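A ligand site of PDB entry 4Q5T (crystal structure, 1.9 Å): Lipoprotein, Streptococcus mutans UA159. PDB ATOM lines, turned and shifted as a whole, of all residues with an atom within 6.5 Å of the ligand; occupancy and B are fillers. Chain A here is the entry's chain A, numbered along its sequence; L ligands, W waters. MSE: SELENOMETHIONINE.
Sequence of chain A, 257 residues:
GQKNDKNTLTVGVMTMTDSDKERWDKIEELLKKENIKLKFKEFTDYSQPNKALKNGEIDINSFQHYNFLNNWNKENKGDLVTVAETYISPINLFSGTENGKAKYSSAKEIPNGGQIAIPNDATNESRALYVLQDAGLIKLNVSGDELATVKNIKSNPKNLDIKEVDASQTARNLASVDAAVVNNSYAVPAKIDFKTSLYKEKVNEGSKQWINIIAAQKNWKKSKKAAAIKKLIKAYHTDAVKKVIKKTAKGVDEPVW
OXT of the ligand sits at hydrogen-bond distance from ND2 of Asn 183.
The side-chain amide oxygen (OD1) of Asn 212 sits close to an oxygen (O) of the ligand (2.9 Å).
NH1 of Arg 127 lies within salt-bridge range of OXT of the ligand (2.9 Å).
N of Asn 212 sits at hydrogen-bond distance from O of Tyr 87.
A ring nitrogen (NE2) of His 65 lies within hydrogen-bond range of the side-chain amide oxygen of Asn 124 (3.2 Å).
The backbone NH (N) of Leu 69 sits close to the side-chain amide oxygen (OE1) of Gln 64 (3.4 Å).
OG of Ser 89 is in hydrogen-bond range of OD1 of Asp 253, at 2.8 Å.
The backbone carbonyl oxygen (O) of Trp 210 lies close to the side-chain amide oxygen (OD1) of Asn 212 (3.3 Å).
The backbone carbonyl oxygen (O) of Ser 89 lies within hydrogen-bond range of the guanidinium group (NH2) of Arg 127, at 3.1 Å.
The side-chain amide nitrogen of Asn 124 is in hydrogen-bond range of the side-chain carboxylate of Asp 121 (2.8 Å).
The side-chain amide nitrogen of Asn 184 is in hydrogen-bond range of the side-chain hydroxyl of Ser 89 (2.8 Å).
Merely in contact with the ligand: Tyr 46 (3.5 Å), Phe 63 (3.3 Å), Gln 64 (3.8 Å), His 65 (3.5 Å), Phe 68 (3.4 Å), Ser 89 (3.7 Å) and Asn 124 (3.6 Å).
Of the 23 residues printed, 10 come within 4 Å of the ligand.
The nearest printed residue that does not touch the ligand is Trp 210 (4.3 Å).
Water W3 lies within hydrogen-bond range of an oxygen (O) of the ligand, the backbone carbonyl oxygen of Trp 210, the backbone NH of Ser 89, the guanidinium group of Arg 127 and the side-chain amide oxygen of Asn 212.
Water W4 lies within hydrogen-bond range of O of Ser 89, OXT of the ligand and N of Asn 184.
Water W2 lies within hydrogen-bond range of O of Phe 63 (2.7 Å), N of the ligand (2.8 Å) and OG of Ser 185 (3.5 Å).
Water W5 lies within hydrogen-bond range of a nitrogen (N) of the ligand, the side-chain hydroxyl of Ser 89, the backbone NH of Ser 185 and the backbone NH of Asn 184.
Water W1 bridges the side-chain hydroxyl of Tyr 87 (2.6 Å) and a nitrogen (N) of the ligand (3.0 Å).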
ATOM      1  N   MET A  14      24.604  -4.102  13.503  1.00  0.00           N
ATOM      2  CA  MET A  14      23.958  -5.338  13.897  1.00  0.00           C
ATOM      3  C   MET A  14      24.937  -6.480  13.710  1.00  0.00           C
ATOM      4  O   MET A  14      25.961  -6.331  13.029  1.00  0.00           O
ATOM      5  CB  MET A  14      22.690  -5.594  13.082  1.00  0.00           C
ATOM      6  CG  MET A  14      21.698  -4.441  13.132  1.00  0.00           C
ATOM      7  SD  MET A  14      21.234  -3.851  14.942  1.00  0.00           S
ATOM      8  CE  MET A  14      20.094  -5.315  15.513  1.00  0.00           C
ATOM      9  N   TYR A  46      17.362  -3.705  17.700  1.00  0.00           N
ATOM     10  CA  TYR A  46      17.338  -2.327  17.180  1.00  0.00           C
ATOM     11  C   TYR A  46      17.258  -1.206  18.238  1.00  0.00           C
ATOM     12  O   TYR A  46      17.449  -0.022  17.930  1.00  0.00           O
ATOM     13  CB  TYR A  46      16.172  -2.123  16.237  1.00  0.00           C
ATOM     14  CG  TYR A  46      16.269  -2.770  14.869  1.00  0.00           C
ATOM     15  CD1 TYR A  46      17.493  -3.148  14.317  1.00  0.00           C
ATOM     16  CD2 TYR A  46      15.122  -2.981  14.117  1.00  0.00           C
ATOM     17  CE1 TYR A  46      17.551  -3.743  13.005  1.00  0.00           C
ATOM     18  CE2 TYR A  46      15.165  -3.567  12.853  1.00  0.00           C
ATOM     19  CZ  TYR A  46      16.378  -3.949  12.308  1.00  0.00           C
ATOM     20  OH  TYR A  46      16.373  -4.506  11.035  1.00  0.00           O
ATOM     21  N   PHE A  63      23.091   1.089  10.975  1.00  0.00           N
ATOM     22  CA  PHE A  63      22.113   0.023  11.203  1.00  0.00           C
ATOM     23  C   PHE A  63      20.666   0.390  10.895  1.00  0.00           C
ATOM     24  O   PHE A  63      19.826  -0.503  10.778  1.00  0.00           O
ATOM     25  CB  PHE A  63      22.175  -0.480  12.646  1.00  0.00           C
ATOM     26  CG  PHE A  63      21.292   0.307  13.592  1.00  0.00           C
ATOM     27  CD1 PHE A  63      21.723   1.542  14.081  1.00  0.00           C
ATOM     28  CD2 PHE A  63      20.071  -0.196  13.995  1.00  0.00           C
ATOM     29  CE1 PHE A  63      20.912   2.273  14.953  1.00  0.00           C
ATOM     30  CE2 PHE A  63      19.246   0.518  14.877  1.00  0.00           C
ATOM     31  CZ  PHE A  63      19.661   1.741  15.364  1.00  0.00           C
ATOM     32  N   GLN A  64      20.401   1.665  10.681  1.00  0.00           N
ATOM     33  CA  GLN A  64      19.014   2.121  10.669  1.00  0.00           C
ATOM     34  C   GLN A  64      18.744   2.984   9.478  1.00  0.00           C
ATOM     35  O   GLN A  64      19.696   3.480   8.849  1.00  0.00           O
ATOM     36  CB  GLN A  64      18.733   2.930  11.952  1.00  0.00           C
ATOM     37  CG  GLN A  64      19.248   4.380  11.908  1.00  0.00           C
ATOM     38  CD  GLN A  64      19.331   5.008  13.307  1.00  0.00           C
ATOM     39  OE1 GLN A  64      18.330   5.144  14.013  1.00  0.00           O
ATOM     40  NE2 GLN A  64      20.544   5.368  13.714  1.00  0.00           N
ATOM     41  N   HIS A  65      17.444   3.165   9.198  1.00  0.00           N
ATOM     42  CA  HIS A  65      16.985   4.140   8.204  1.00  0.00           C
ATOM     43  C   HIS A  65      16.536   5.462   8.848  1.00  0.00           C
ATOM     44  O   HIS A  65      16.371   5.538  10.063  1.00  0.00           O
ATOM     45  CB  HIS A  65      15.908   3.569   7.241  1.00  0.00           C
ATOM     46  CG  HIS A  65      14.760   2.906   7.908  1.00  0.00           C
ATOM     47  ND1 HIS A  65      13.909   3.575   8.771  1.00  0.00           N
ATOM     48  CD2 HIS A  65      14.275   1.638   7.821  1.00  0.00           C
ATOM     49  CE1 HIS A  65      12.986   2.734   9.211  1.00  0.00           C
ATOM     50  NE2 HIS A  65      13.191   1.548   8.649  1.00  0.00           N
ATOM     51  N   PHE A  68      13.535   5.402  11.305  1.00  0.00           N
ATOM     52  CA  PHE A  68      13.826   4.827  12.590  1.00  0.00           C
ATOM     53  C   PHE A  68      14.553   5.889  13.404  1.00  0.00           C
ATOM     54  O   PHE A  68      14.179   6.117  14.584  1.00  0.00           O
ATOM     55  CB  PHE A  68      14.650   3.545  12.461  1.00  0.00           C
ATOM     56  CG  PHE A  68      14.834   2.823  13.784  1.00  0.00           C
ATOM     57  CD1 PHE A  68      15.864   3.187  14.636  1.00  0.00           C
ATOM     58  CD2 PHE A  68      13.960   1.822  14.164  1.00  0.00           C
ATOM     59  CE1 PHE A  68      16.037   2.531  15.860  1.00  0.00           C
ATOM     60  CE2 PHE A  68      14.128   1.160  15.365  1.00  0.00           C
ATOM     61  CZ  PHE A  68      15.162   1.534  16.227  1.00  0.00           C
ATOM     62  N   LEU A  69      15.520   6.571  12.786  1.00  0.00           N
ATOM     63  CA  LEU A  69      16.288   7.607  13.477  1.00  0.00           C
ATOM     64  C   LEU A  69      15.395   8.713  14.017  1.00  0.00           C
ATOM     65  O   LEU A  69      15.430   9.001  15.191  1.00  0.00           O
ATOM     66  CB  LEU A  69      17.344   8.240  12.571  1.00  0.00           C
ATOM     67  CG  LEU A  69      18.188   9.309  13.274  1.00  0.00           C
ATOM     68  CD1 LEU A  69      18.915   8.718  14.453  1.00  0.00           C
ATOM     69  CD2 LEU A  69      19.188   9.941  12.320  1.00  0.00           C
ATOM     70  N   TYR A  87      22.771   2.295   2.058  1.00  0.00           N
ATOM     71  CA  TYR A  87      22.021   1.483   1.100  1.00  0.00           C
ATOM     72  C   TYR A  87      20.551   1.475   1.502  1.00  0.00           C
ATOM     73  O   TYR A  87      20.183   1.832   2.640  1.00  0.00           O
ATOM     74  CB  TYR A  87      22.591   0.072   1.086  1.00  0.00           C
ATOM     75  CG  TYR A  87      22.703  -0.544   2.475  1.00  0.00           C
ATOM     76  CD1 TYR A  87      23.833  -0.363   3.242  1.00  0.00           C
ATOM     77  CD2 TYR A  87      21.679  -1.313   3.005  1.00  0.00           C
ATOM     78  CE1 TYR A  87      23.943  -0.902   4.500  1.00  0.00           C
ATOM     79  CE2 TYR A  87      21.777  -1.855   4.270  1.00  0.00           C
ATOM     80  CZ  TYR A  87      22.907  -1.640   5.024  1.00  0.00           C
ATOM     81  OH  TYR A  87      23.036  -2.169   6.276  1.00  0.00           O
ATOM     82  N   ILE A  88      19.715   1.066   0.570  1.00  0.00           N
ATOM     83  CA  ILE A  88      18.333   0.733   0.874  1.00  0.00           C
ATOM     84  C   ILE A  88      18.180  -0.796   0.858  1.00  0.00           C
ATOM     85  O   ILE A  88      18.930  -1.487   0.152  1.00  0.00           O
ATOM     86  CB  ILE A  88      17.312   1.437  -0.040  1.00  0.00           C
ATOM     87  CG1 ILE A  88      15.893   1.100   0.422  1.00  0.00           C
ATOM     88  CG2 ILE A  88      17.477   1.017  -1.515  1.00  0.00           C
ATOM     89  CD1 ILE A  88      14.865   2.047  -0.084  1.00  0.00           C
ATOM     90  N   SER A  89      17.272  -1.309   1.686  1.00  0.00           N
ATOM     91  CA  SER A  89      17.117  -2.740   1.901  1.00  0.00           C
ATOM     92  C   SER A  89      15.656  -3.180   1.882  1.00  0.00           C
ATOM     93  O   SER A  89      15.056  -3.400   2.945  1.00  0.00           O
ATOM     94  CB  SER A  89      17.815  -3.176   3.195  1.00  0.00           C
ATOM     95  OG  SER A  89      17.911  -4.589   3.299  1.00  0.00           O
ATOM     96  N   PRO A  90      15.067  -3.290   0.657  1.00  0.00           N
ATOM     97  CA  PRO A  90      13.640  -3.575   0.461  1.00  0.00           C
ATOM     98  C   PRO A  90      13.229  -4.807   1.216  1.00  0.00           C
ATOM     99  O   PRO A  90      13.881  -5.835   1.104  1.00  0.00           O
ATOM    100  CB  PRO A  90      13.501  -3.810  -1.045  1.00  0.00           C
ATOM    101  CG  PRO A  90      14.671  -3.125  -1.640  1.00  0.00           C
ATOM    102  CD  PRO A  90      15.771  -3.153  -0.616  1.00  0.00           C
ATOM    103  N   ILE A  91      12.171  -4.678   1.991  1.00  0.00           N
ATOM    104  CA  ILE A  91      11.797  -5.678   2.947  1.00  0.00           C
ATOM    105  C   ILE A  91      10.804  -6.652   2.292  1.00  0.00           C
ATOM    106  O   ILE A  91      10.163  -6.314   1.289  1.00  0.00           O
ATOM    107  CB  ILE A  91      11.200  -4.970   4.202  1.00  0.00           C
ATOM    108  CG1 ILE A  91      11.189  -5.892   5.413  1.00  0.00           C
ATOM    109  CG2 ILE A  91       9.810  -4.453   3.913  1.00  0.00           C
ATOM    110  CD1 ILE A  91      10.944  -5.102   6.732  1.00  0.00           C
ATOM    111  N   ASP A 121       8.181  -1.699  16.499  1.00  0.00           N
ATOM    112  CA  ASP A 121       8.670  -0.325  16.597  1.00  0.00           C
ATOM    113  C   ASP A 121       7.867   0.498  15.591  1.00  0.00           C
ATOM    114  O   ASP A 121       7.531   0.031  14.527  1.00  0.00           O
ATOM    115  CB  ASP A 121      10.178  -0.263  16.319  1.00  0.00           C
ATOM    116  CG  ASP A 121      10.537  -0.724  14.890  1.00  0.00           C
ATOM    117  OD1 ASP A 121      10.604  -1.955  14.674  1.00  0.00           O
ATOM    118  OD2 ASP A 121      10.711   0.124  14.000  1.00  0.00           O
ATOM    119  N   THR A 123       8.171   2.713  13.179  1.00  0.00           N
ATOM    120  CA  THR A 123       8.434   2.911  11.751  1.00  0.00           C
ATOM    121  C   THR A 123       8.439   1.602  10.968  1.00  0.00           C
ATOM    122  O   THR A 123       7.898   1.537   9.864  1.00  0.00           O
ATOM    123  CB  THR A 123       9.750   3.742  11.507  1.00  0.00           C
ATOM    124  OG1 THR A 123      10.902   2.974  11.879  1.00  0.00           O
ATOM    125  CG2 THR A 123       9.731   5.008  12.345  1.00  0.00           C
ATOM    126  N   ASN A 124       9.036   0.539  11.502  1.00  0.00           N
ATOM    127  CA  ASN A 124       8.998  -0.748  10.795  1.00  0.00           C
ATOM    128  C   ASN A 124       7.639  -1.420  10.905  1.00  0.00           C
ATOM    129  O   ASN A 124       7.265  -2.166  10.027  1.00  0.00           O
ATOM    130  CB  ASN A 124      10.128  -1.679  11.238  1.00  0.00           C
ATOM    131  CG  ASN A 124      11.506  -1.147  10.839  1.00  0.00           C
ATOM    132  OD1 ASN A 124      11.843  -1.123   9.656  1.00  0.00           O
ATOM    133  ND2 ASN A 124      12.293  -0.718  11.811  1.00  0.00           N
ATOM    134  N   ARG A 127       5.874   0.327   8.196  1.00  0.00           N
ATOM    135  CA  ARG A 127       6.405  -0.171   6.928  1.00  0.00           C
ATOM    136  C   ARG A 127       5.737  -1.500   6.525  1.00  0.00           C
ATOM    137  O   ARG A 127       5.370  -1.700   5.352  1.00  0.00           O
ATOM    138  CB  ARG A 127       7.917  -0.357   7.064  1.00  0.00           C
ATOM    139  CG  ARG A 127       8.605  -0.732   5.813  1.00  0.00           C
ATOM    140  CD  ARG A 127      10.088  -0.839   6.116  1.00  0.00           C
ATOM    141  NE  ARG A 127      10.886  -0.995   4.931  1.00  0.00           N
ATOM    142  CZ  ARG A 127      12.208  -1.151   4.957  1.00  0.00           C
ATOM    143  NH1 ARG A 127      12.846  -1.200   6.122  1.00  0.00           N
ATOM    144  NH2 ARG A 127      12.875  -1.318   3.831  1.00  0.00           N
ATOM    145  N   ASN A 183      12.832  -7.688   8.465  1.00  0.00           N
ATOM    146  CA  ASN A 183      13.952  -6.890   8.004  1.00  0.00           C
ATOM    147  C   ASN A 183      15.077  -7.796   7.581  1.00  0.00           C
ATOM    148  O   ASN A 183      15.354  -8.794   8.234  1.00  0.00           O
ATOM    149  CB  ASN A 183      14.463  -5.962   9.113  1.00  0.00           C
ATOM    150  CG  ASN A 183      13.416  -4.978   9.613  1.00  0.00           C
ATOM    151  OD1 ASN A 183      12.604  -5.312  10.480  1.00  0.00           O
ATOM    152  ND2 ASN A 183      13.415  -3.762   9.056  1.00  0.00           N
ATOM    153  N   ASN A 184      15.766  -7.441   6.500  1.00  0.00           N
ATOM    154  CA  ASN A 184      16.859  -8.274   5.991  1.00  0.00           C
ATOM    155  C   ASN A 184      18.008  -8.491   6.953  1.00  0.00           C
ATOM    156  O   ASN A 184      18.658  -9.538   6.939  1.00  0.00           O
ATOM    157  CB  ASN A 184      17.371  -7.714   4.653  1.00  0.00           C
ATOM    158  CG  ASN A 184      16.325  -7.818   3.562  1.00  0.00           C
ATOM    159  OD1 ASN A 184      15.692  -8.875   3.402  1.00  0.00           O
ATOM    160  ND2 ASN A 184      16.118  -6.740   2.809  1.00  0.00           N
ATOM    161  N   SER A 185      18.265  -7.507   7.832  1.00  0.00           N
ATOM    162  CA  SER A 185      19.313  -7.654   8.816  1.00  0.00           C
ATOM    163  C   SER A 185      19.085  -8.893   9.681  1.00  0.00           C
ATOM    164  O   SER A 185      20.041  -9.512  10.188  1.00  0.00           O
ATOM    165  CB  SER A 185      19.421  -6.371   9.672  1.00  0.00           C
ATOM    166  OG  SER A 185      18.265  -6.146  10.484  1.00  0.00           O
ATOM    167  N   TRP A 210      13.319   4.894   3.897  1.00  0.00           N
ATOM    168  CA  TRP A 210      13.872   3.589   4.243  1.00  0.00           C
ATOM    169  C   TRP A 210      15.355   3.477   3.877  1.00  0.00           C
ATOM    170  O   TRP A 210      15.963   2.413   4.046  1.00  0.00           O
ATOM    171  CB  TRP A 210      13.114   2.424   3.578  1.00  0.00           C
ATOM    172  CG  TRP A 210      11.617   2.566   3.650  1.00  0.00           C
ATOM    173  CD1 TRP A 210      10.744   2.563   2.592  1.00  0.00           C
ATOM    174  CD2 TRP A 210      10.826   2.732   4.823  1.00  0.00           C
ATOM    175  NE1 TRP A 210       9.449   2.728   3.048  1.00  0.00           N
ATOM    176  CE2 TRP A 210       9.474   2.829   4.411  1.00  0.00           C
ATOM    177  CE3 TRP A 210      11.123   2.817   6.189  1.00  0.00           C
ATOM    178  CZ2 TRP A 210       8.425   3.014   5.320  1.00  0.00           C
ATOM    179  CZ3 TRP A 210      10.079   2.999   7.090  1.00  0.00           C
ATOM    180  CH2 TRP A 210       8.751   3.086   6.658  1.00  0.00           C
ATOM    181  N   ILE A 211      15.958   4.562   3.388  1.00  0.00           N
ATOM    182  CA  ILE A 211      17.397   4.565   3.112  1.00  0.00           C
ATOM    183  C   ILE A 211      18.147   4.455   4.443  1.00  0.00           C
ATOM    184  O   ILE A 211      17.866   5.176   5.388  1.00  0.00           O
ATOM    185  CB  ILE A 211      17.830   5.853   2.336  1.00  0.00           C
ATOM    186  CG1 ILE A 211      17.202   5.810   0.942  1.00  0.00           C
ATOM    187  CG2 ILE A 211      19.359   5.974   2.267  1.00  0.00           C
ATOM    188  CD1 ILE A 211      17.590   6.944   0.026  1.00  0.00           C
ATOM    189  N   ASN A 212      19.083   3.518   4.522  1.00  0.00           N
ATOM    190  CA  ASN A 212      19.876   3.401   5.713  1.00  0.00           C
ATOM    191  C   ASN A 212      20.965   4.484   5.749  1.00  0.00           C
ATOM    192  O   ASN A 212      21.356   5.050   4.711  1.00  0.00           O
ATOM    193  CB  ASN A 212      20.496   2.027   5.847  1.00  0.00           C
ATOM    194  CG  ASN A 212      19.479   0.962   6.219  1.00  0.00           C
ATOM    195  OD1 ASN A 212      18.389   0.924   5.685  1.00  0.00           O
ATOM    196  ND2 ASN A 212      19.867   0.084   7.100  1.00  0.00           N
ATOM    197  N   ASP A 253      20.510  -5.584  -0.299  1.00  0.00           N
ATOM    198  CA  ASP A 253      20.941  -4.220  -0.051  1.00  0.00           C
ATOM    199  C   ASP A 253      21.411  -3.553  -1.353  1.00  0.00           C
ATOM    200  O   ASP A 253      22.219  -4.143  -2.115  1.00  0.00           O
ATOM    201  CB  ASP A 253      22.128  -4.165   0.902  1.00  0.00           C
ATOM    202  CG  ASP A 253      21.842  -4.752   2.273  1.00  0.00           C
ATOM    203  OD1 ASP A 253      20.653  -4.862   2.667  1.00  0.00           O
ATOM    204  OD2 ASP A 253      22.868  -5.068   2.970  1.00  0.00           O
HETATM  205  N   MSE L   1      18.580  -2.361   7.881  1.00  0.00           N
HETATM  206  CA  MSE L   1      17.162  -2.223   8.280  1.00  0.00           C
HETATM  207  C   MSE L   1      16.254  -2.027   7.077  1.00  0.00           C
HETATM  208  O   MSE L   1      16.614  -1.280   6.112  1.00  0.00           O
HETATM  209  OXT MSE L   1      15.154  -2.640   7.066  1.00  0.00           O
HETATM  210  CB  MSE L   1      16.991  -1.021   9.244  1.00  0.00           C
HETATM  211  CG  MSE L   1      15.613  -0.930   9.862  1.00  0.00           C
HETATM  212 SE   MSE L   1      15.568   0.544  11.158  1.00  0.00          SE
HETATM  213  CE  MSE L   1      16.690  -0.252  12.532  1.00  0.00           C
HETATM  214  O   HOH W   1      21.140  -3.706   7.197  1.00  0.00           O
HETATM  215  O   HOH W   2      19.973  -3.138  10.181  1.00  0.00           O
HETATM  216  O   HOH W   3      15.767  -0.358   3.976  1.00  0.00           O
HETATM  217  O   HOH W   4      15.211  -4.697   5.288  1.00  0.00           O
HETATM  218  O   HOH W   5      17.806  -4.721   6.395  1.00  0.00           O
